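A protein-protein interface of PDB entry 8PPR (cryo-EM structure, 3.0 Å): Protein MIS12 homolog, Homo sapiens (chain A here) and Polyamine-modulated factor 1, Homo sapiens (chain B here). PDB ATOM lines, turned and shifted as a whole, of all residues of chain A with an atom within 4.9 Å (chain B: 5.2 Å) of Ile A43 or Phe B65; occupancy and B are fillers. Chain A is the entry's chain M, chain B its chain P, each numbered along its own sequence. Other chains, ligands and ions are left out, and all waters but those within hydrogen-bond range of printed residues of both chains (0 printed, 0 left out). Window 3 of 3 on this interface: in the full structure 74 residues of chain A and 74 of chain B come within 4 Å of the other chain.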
ATOM      1  N   VAL A  39       7.194   3.230  -3.716  1.00  0.00           N
ATOM      2  CA  VAL A  39       6.648   2.162  -2.885  1.00  0.00           C
ATOM      3  C   VAL A  39       5.955   2.738  -1.655  1.00  0.00           C
ATOM      4  O   VAL A  39       4.897   2.251  -1.235  1.00  0.00           O
ATOM      5  CB  VAL A  39       7.759   1.167  -2.508  1.00  0.00           C
ATOM      6  CG1 VAL A  39       7.252   0.154  -1.500  1.00  0.00           C
ATOM      7  CG2 VAL A  39       8.271   0.470  -3.753  1.00  0.00           C
ATOM      8  N   GLU A  40       6.538   3.781  -1.055  1.00  0.00           N
ATOM      9  CA  GLU A  40       5.901   4.426   0.090  1.00  0.00           C
ATOM     10  C   GLU A  40       4.559   5.034  -0.295  1.00  0.00           C
ATOM     11  O   GLU A  40       3.575   4.911   0.443  1.00  0.00           O
ATOM     12  CB  GLU A  40       6.823   5.498   0.672  1.00  0.00           C
ATOM     13  CG  GLU A  40       6.141   6.401   1.690  1.00  0.00           C
ATOM     14  CD  GLU A  40       6.982   7.601   2.076  1.00  0.00           C
ATOM     15  OE1 GLU A  40       8.224   7.523   1.971  1.00  0.00           O
ATOM     16  OE2 GLU A  40       6.397   8.624   2.488  1.00  0.00           O
ATOM     17  N   GLN A  41       4.500   5.699  -1.448  1.00  0.00           N
ATOM     18  CA  GLN A  41       3.238   6.269  -1.907  1.00  0.00           C
ATOM     19  C   GLN A  41       2.209   5.175  -2.153  1.00  0.00           C
ATOM     20  O   GLN A  41       1.027   5.335  -1.823  1.00  0.00           O
ATOM     21  CB  GLN A  41       3.466   7.097  -3.170  1.00  0.00           C
ATOM     22  CG  GLN A  41       4.231   8.388  -2.932  1.00  0.00           C
ATOM     23  CD  GLN A  41       4.589   9.096  -4.222  1.00  0.00           C
ATOM     24  OE1 GLN A  41       4.251   8.633  -5.311  1.00  0.00           O
ATOM     25  NE2 GLN A  41       5.277  10.227  -4.106  1.00  0.00           N
ATOM     26  N   VAL A  42       2.645   4.048  -2.721  1.00  0.00           N
ATOM     27  CA  VAL A  42       1.738   2.926  -2.953  1.00  0.00           C
ATOM     28  C   VAL A  42       1.191   2.401  -1.631  1.00  0.00           C
ATOM     29  O   VAL A  42      -0.009   2.130  -1.500  1.00  0.00           O
ATOM     30  CB  VAL A  42       2.451   1.816  -3.746  1.00  0.00           C
ATOM     31  CG1 VAL A  42       1.686   0.508  -3.635  1.00  0.00           C
ATOM     32  CG2 VAL A  42       2.611   2.222  -5.203  1.00  0.00           C
ATOM     33  N   ILE A  43       2.060   2.242  -0.632  1.00  0.00           N
ATOM     34  CA  ILE A  43       1.610   1.665   0.632  1.00  0.00           C
ATOM     35  C   ILE A  43       0.683   2.632   1.368  1.00  0.00           C
ATOM     36  O   ILE A  43      -0.307   2.212   1.980  1.00  0.00           O
ATOM     37  CB  ILE A  43       2.812   1.223   1.495  1.00  0.00           C
ATOM     38  CG1 ILE A  43       2.373   0.188   2.532  1.00  0.00           C
ATOM     39  CG2 ILE A  43       3.487   2.390   2.188  1.00  0.00           C
ATOM     40  CD1 ILE A  43       3.520  -0.387   3.336  1.00  0.00           C
ATOM     41  N   LEU A  44       0.961   3.938   1.295  1.00  0.00           N
ATOM     42  CA  LEU A  44       0.051   4.906   1.906  1.00  0.00           C
ATOM     43  C   LEU A  44      -1.291   4.959   1.182  1.00  0.00           C
ATOM     44  O   LEU A  44      -2.335   5.096   1.827  1.00  0.00           O
ATOM     45  CB  LEU A  44       0.689   6.295   1.977  1.00  0.00           C
ATOM     46  CG  LEU A  44       1.623   6.634   3.151  1.00  0.00           C
ATOM     47  CD1 LEU A  44       0.830   6.598   4.451  1.00  0.00           C
ATOM     48  CD2 LEU A  44       2.830   5.727   3.264  1.00  0.00           C
ATOM     49  N   LYS A  45      -1.299   4.850  -0.149  1.00  0.00           N
ATOM     50  CA  LYS A  45      -2.585   4.844  -0.842  1.00  0.00           C
ATOM     51  C   LYS A  45      -3.359   3.559  -0.564  1.00  0.00           C
ATOM     52  O   LYS A  45      -4.594   3.584  -0.492  1.00  0.00           O
ATOM     53  CB  LYS A  45      -2.389   5.060  -2.346  1.00  0.00           C
ATOM     54  CG  LYS A  45      -1.995   3.828  -3.141  1.00  0.00           C
ATOM     55  CD  LYS A  45      -1.689   4.182  -4.587  1.00  0.00           C
ATOM     56  CE  LYS A  45      -1.852   2.979  -5.502  1.00  0.00           C
ATOM     57  NZ  LYS A  45      -0.808   1.948  -5.259  1.00  0.00           N
ATOM     58  N   LYS A  46      -2.659   2.436  -0.384  1.00  0.00           N
ATOM     59  CA  LYS A  46      -3.329   1.198   0.003  1.00  0.00           C
ATOM     60  C   LYS A  46      -3.913   1.307   1.405  1.00  0.00           C
ATOM     61  O   LYS A  46      -5.019   0.816   1.667  1.00  0.00           O
ATOM     62  CB  LYS A  46      -2.354   0.024  -0.085  1.00  0.00           C
ATOM     63  CG  LYS A  46      -2.052  -0.421  -1.508  1.00  0.00           C
ATOM     64  CD  LYS A  46      -3.329  -0.700  -2.282  1.00  0.00           C
ATOM     65  CE  LYS A  46      -3.038  -1.445  -3.575  1.00  0.00           C
ATOM     66  NZ  LYS A  46      -1.975  -2.472  -3.408  1.00  0.00           N
ATOM     67  N   LEU A  47      -3.179   1.940   2.323  1.00  0.00           N
ATOM     68  CA  LEU A  47      -3.706   2.174   3.665  1.00  0.00           C
ATOM     69  C   LEU A  47      -4.912   3.104   3.626  1.00  0.00           C
ATOM     70  O   LEU A  47      -5.872   2.924   4.384  1.00  0.00           O
ATOM     71  CB  LEU A  47      -2.609   2.748   4.562  1.00  0.00           C
ATOM     72  CG  LEU A  47      -1.649   1.730   5.177  1.00  0.00           C
ATOM     73  CD1 LEU A  47      -0.435   2.425   5.777  1.00  0.00           C
ATOM     74  CD2 LEU A  47      -2.368   0.895   6.222  1.00  0.00           C
ATOM     75  N   ILE A  55      -2.583   2.125  10.848  1.00  0.00           N
ATOM     76  CA  ILE A  55      -1.169   2.364  10.567  1.00  0.00           C
ATOM     77  C   ILE A  55      -1.017   3.848  10.242  1.00  0.00           C
ATOM     78  O   ILE A  55      -1.297   4.283   9.124  1.00  0.00           O
ATOM     79  CB  ILE A  55      -0.653   1.479   9.432  1.00  0.00           C
ATOM     80  CG1 ILE A  55      -1.069   0.026   9.662  1.00  0.00           C
ATOM     81  CG2 ILE A  55       0.861   1.593   9.313  1.00  0.00           C
ATOM     82  CD1 ILE A  55      -0.572  -0.550  10.969  1.00  0.00           C
ATOM     83  N   ILE A  60       4.668   4.348   9.523  1.00  0.00           N
ATOM     84  CA  ILE A  60       5.172   3.800   8.270  1.00  0.00           C
ATOM     85  C   ILE A  60       6.351   4.622   7.765  1.00  0.00           C
ATOM     86  O   ILE A  60       7.292   4.077   7.180  1.00  0.00           O
ATOM     87  CB  ILE A  60       4.043   3.695   7.226  1.00  0.00           C
ATOM     88  CG1 ILE A  60       4.525   2.929   5.992  1.00  0.00           C
ATOM     89  CG2 ILE A  60       3.519   5.066   6.836  1.00  0.00           C
ATOM     90  CD1 ILE A  60       5.003   1.526   6.293  1.00  0.00           C
ATOM     91  N   TYR B  62       8.901  -3.580   8.318  1.00  0.00           N
ATOM     92  CA  TYR B  62       7.545  -3.123   8.032  1.00  0.00           C
ATOM     93  C   TYR B  62       6.509  -3.998   8.729  1.00  0.00           C
ATOM     94  O   TYR B  62       5.455  -4.308   8.171  1.00  0.00           O
ATOM     95  CB  TYR B  62       7.291  -3.088   6.529  1.00  0.00           C
ATOM     96  CG  TYR B  62       8.122  -2.062   5.795  1.00  0.00           C
ATOM     97  CD1 TYR B  62       8.702  -0.998   6.472  1.00  0.00           C
ATOM     98  CD2 TYR B  62       8.327  -2.155   4.427  1.00  0.00           C
ATOM     99  CE1 TYR B  62       9.464  -0.058   5.808  1.00  0.00           C
ATOM    100  CE2 TYR B  62       9.087  -1.220   3.754  1.00  0.00           C
ATOM    101  CZ  TYR B  62       9.653  -0.174   4.448  1.00  0.00           C
ATOM    102  OH  TYR B  62      10.411   0.759   3.780  1.00  0.00           O
ATOM    103  N   LYS B  63       6.805  -4.407   9.965  1.00  0.00           N
ATOM    104  CA  LYS B  63       5.902  -5.278  10.707  1.00  0.00           C
ATOM    105  C   LYS B  63       4.565  -4.615  11.009  1.00  0.00           C
ATOM    106  O   LYS B  63       3.572  -5.320  11.215  1.00  0.00           O
ATOM    107  CB  LYS B  63       6.559  -5.722  12.015  1.00  0.00           C
ATOM    108  CG  LYS B  63       7.070  -4.568  12.865  1.00  0.00           C
ATOM    109  CD  LYS B  63       7.117  -4.936  14.340  1.00  0.00           C
ATOM    110  CE  LYS B  63       8.066  -6.094  14.596  1.00  0.00           C
ATOM    111  NZ  LYS B  63       9.490  -5.674  14.480  1.00  0.00           N
ATOM    112  N   CYS B  64       4.516  -3.281  11.047  1.00  0.00           N
ATOM    113  CA  CYS B  64       3.267  -2.595  11.364  1.00  0.00           C
ATOM    114  C   CYS B  64       2.211  -2.857  10.297  1.00  0.00           C
ATOM    115  O   CYS B  64       1.088  -3.274  10.606  1.00  0.00           O
ATOM    116  CB  CYS B  64       3.519  -1.094  11.518  1.00  0.00           C
ATOM    117  SG  CYS B  64       4.086  -0.273  10.010  1.00  0.00           S
ATOM    118  N   PHE B  65       2.555  -2.623   9.030  1.00  0.00           N
ATOM    119  CA  PHE B  65       1.616  -2.876   7.945  1.00  0.00           C
ATOM    120  C   PHE B  65       1.494  -4.359   7.620  1.00  0.00           C
ATOM    121  O   PHE B  65       0.439  -4.801   7.152  1.00  0.00           O
ATOM    122  CB  PHE B  65       2.032  -2.108   6.691  1.00  0.00           C
ATOM    123  CG  PHE B  65       1.118  -2.328   5.521  1.00  0.00           C
ATOM    124  CD1 PHE B  65      -0.129  -1.730   5.475  1.00  0.00           C
ATOM    125  CD2 PHE B  65       1.502  -3.147   4.474  1.00  0.00           C
ATOM    126  CE1 PHE B  65      -0.974  -1.938   4.401  1.00  0.00           C
ATOM    127  CE2 PHE B  65       0.663  -3.359   3.400  1.00  0.00           C
ATOM    128  CZ  PHE B  65      -0.576  -2.753   3.362  1.00  0.00           C
ATOM    129  N   TYR B  66       2.555  -5.135   7.854  1.00  0.00           N
ATOM    130  CA  TYR B  66       2.537  -6.550   7.496  1.00  0.00           C
ATOM    131  C   TYR B  66       1.506  -7.326   8.303  1.00  0.00           C
ATOM    132  O   TYR B  66       1.016  -8.365   7.847  1.00  0.00           O
ATOM    133  CB  TYR B  66       3.927  -7.150   7.692  1.00  0.00           C
ATOM    134  CG  TYR B  66       4.112  -8.507   7.059  1.00  0.00           C
ATOM    135  CD1 TYR B  66       4.439  -8.628   5.714  1.00  0.00           C
ATOM    136  CD2 TYR B  66       3.974  -9.668   7.807  1.00  0.00           C
ATOM    137  CE1 TYR B  66       4.618  -9.867   5.133  1.00  0.00           C
ATOM    138  CE2 TYR B  66       4.149 -10.912   7.234  1.00  0.00           C
ATOM    139  CZ  TYR B  66       4.474 -11.005   5.897  1.00  0.00           C
ATOM    140  OH  TYR B  66       4.646 -12.243   5.320  1.00  0.00           O
ATOM    141  N   GLN B  67       1.168  -6.846   9.502  1.00  0.00           N
ATOM    142  CA  GLN B  67       0.173  -7.514  10.332  1.00  0.00           C
ATOM    143  C   GLN B  67      -1.238  -7.402   9.771  1.00  0.00           C
ATOM    144  O   GLN B  67      -2.134  -8.106  10.250  1.00  0.00           O
ATOM    145  CB  GLN B  67       0.210  -6.944  11.751  1.00  0.00           C
ATOM    146  CG  GLN B  67       1.360  -7.462  12.599  1.00  0.00           C
ATOM    147  CD  GLN B  67       1.670  -6.552  13.770  1.00  0.00           C
ATOM    148  OE1 GLN B  67       1.168  -5.431  13.850  1.00  0.00           O
ATOM    149  NE2 GLN B  67       2.501  -7.032  14.689  1.00  0.00           N
ATOM    150  N   LEU B  68      -1.457  -6.545   8.774  1.00  0.00           N
ATOM    151  CA  LEU B  68      -2.780  -6.338   8.192  1.00  0.00           C
ATOM    152  C   LEU B  68      -2.992  -7.196   6.949  1.00  0.00           C
ATOM    153  O   LEU B  68      -3.958  -7.961   6.873  1.00  0.00           O
ATOM    154  CB  LEU B  68      -2.977  -4.854   7.858  1.00  0.00           C
ATOM    155  CG  LEU B  68      -3.565  -3.964   8.955  1.00  0.00           C
ATOM    156  CD1 LEU B  68      -2.539  -3.693  10.048  1.00  0.00           C
ATOM    157  CD2 LEU B  68      -4.080  -2.662   8.365  1.00  0.00           C
ATOM    158  N   GLN B  69      -2.097  -7.083   5.969  1.00  0.00           N
ATOM    159  CA  GLN B  69      -2.180  -7.855   4.730  1.00  0.00           C
ATOM    160  C   GLN B  69      -0.767  -8.224   4.306  1.00  0.00           C
ATOM    161  O   GLN B  69      -0.076  -7.444   3.639  1.00  0.00           O
ATOM    162  CB  GLN B  69      -2.896  -7.069   3.629  1.00  0.00           C
ATOM    163  CG  GLN B  69      -4.416  -7.182   3.653  1.00  0.00           C
ATOM    164  CD  GLN B  69      -4.912  -8.574   3.308  1.00  0.00           C
ATOM    165  OE1 GLN B  69      -4.203  -9.358   2.679  1.00  0.00           O
ATOM    166  NE2 GLN B  69      -6.134  -8.887   3.721  1.00  0.00           N
ATOM    167  N   MET B  72      -0.140  -8.407  -0.035  1.00  0.00           N
ATOM    168  CA  MET B  72       0.116  -7.194  -0.800  1.00  0.00           C
ATOM    169  C   MET B  72       1.467  -6.607  -0.417  1.00  0.00           C
ATOM    170  O   MET B  72       2.166  -6.048  -1.270  1.00  0.00           O
ATOM    171  CB  MET B  72      -1.034  -6.204  -0.578  1.00  0.00           C
ATOM    172  CG  MET B  72      -1.109  -4.980  -1.505  1.00  0.00           C
ATOM    173  SD  MET B  72       0.286  -3.852  -1.695  1.00  0.00           S
ATOM    174  CE  MET B  72       0.455  -3.219  -0.032  1.00  0.00           C
ATOM    175  N   THR B  73       1.874  -6.783   0.842  1.00  0.00           N
ATOM    176  CA  THR B  73       3.228  -6.425   1.245  1.00  0.00           C
ATOM    177  C   THR B  73       4.262  -7.225   0.456  1.00  0.00           C
ATOM    178  O   THR B  73       5.294  -6.685   0.039  1.00  0.00           O
ATOM    179  CB  THR B  73       3.397  -6.652   2.747  1.00  0.00           C
ATOM    180  OG1 THR B  73       2.298  -6.058   3.447  1.00  0.00           O
ATOM    181  CG2 THR B  73       4.683  -6.023   3.240  1.00  0.00           C
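SD of Met B72 is in hydrogen-bond range of NZ of Lys A46, at 3.2 Å.
Phe B65 touches Ile A43.
Phe B65 touches Leu A47 (CD1 to CD2, 3.5 Å).
CD1 of Ile A55 touches O of Cys B64, 3.2 Å away.
Leu B68 touches Ile A55.
Of the 10 printed residues of chain B, 4 touch a printed residue of chain A.
Printed residues of chain B that touch a printed residue of chain A: Cys B64, Phe B65, Leu B68 and Met B72.
Of the 11 printed residues of chain A, 4 touch a printed residue of chain B.
Printed residues of chain A that touch a printed residue of chain B: Ile A43, Lys A46, Leu A47 and Ile A55.
Among the printed residues, 5 pairs touch across the chains.
Of the printed residues of chain B, Lys A46 touches Met B72 (3.2 Å).
Printed residues of chain B within 4 Å of Ile A55: Cys B64 and Leu B68.
Of the printed residues of chain A, Cys B64 touches Ile A55.
Phe B65 touches two residues of chain A.
Gln B67 touches none of the printed residues of chain A.
Printed residues of chain A within 4 Å of Met B72: Lys A46 (3.2 Å).
The nearest residue of chain B that does not touch Ile A43 is Met B72 (4.7 Å).
The nearest residue of chain A that does not touch Phe B65 is Ile A55 (4.2 Å).
The nearest printed residue of chain B that does not touch Ile A55 is Phe B65 (4.2 Å).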
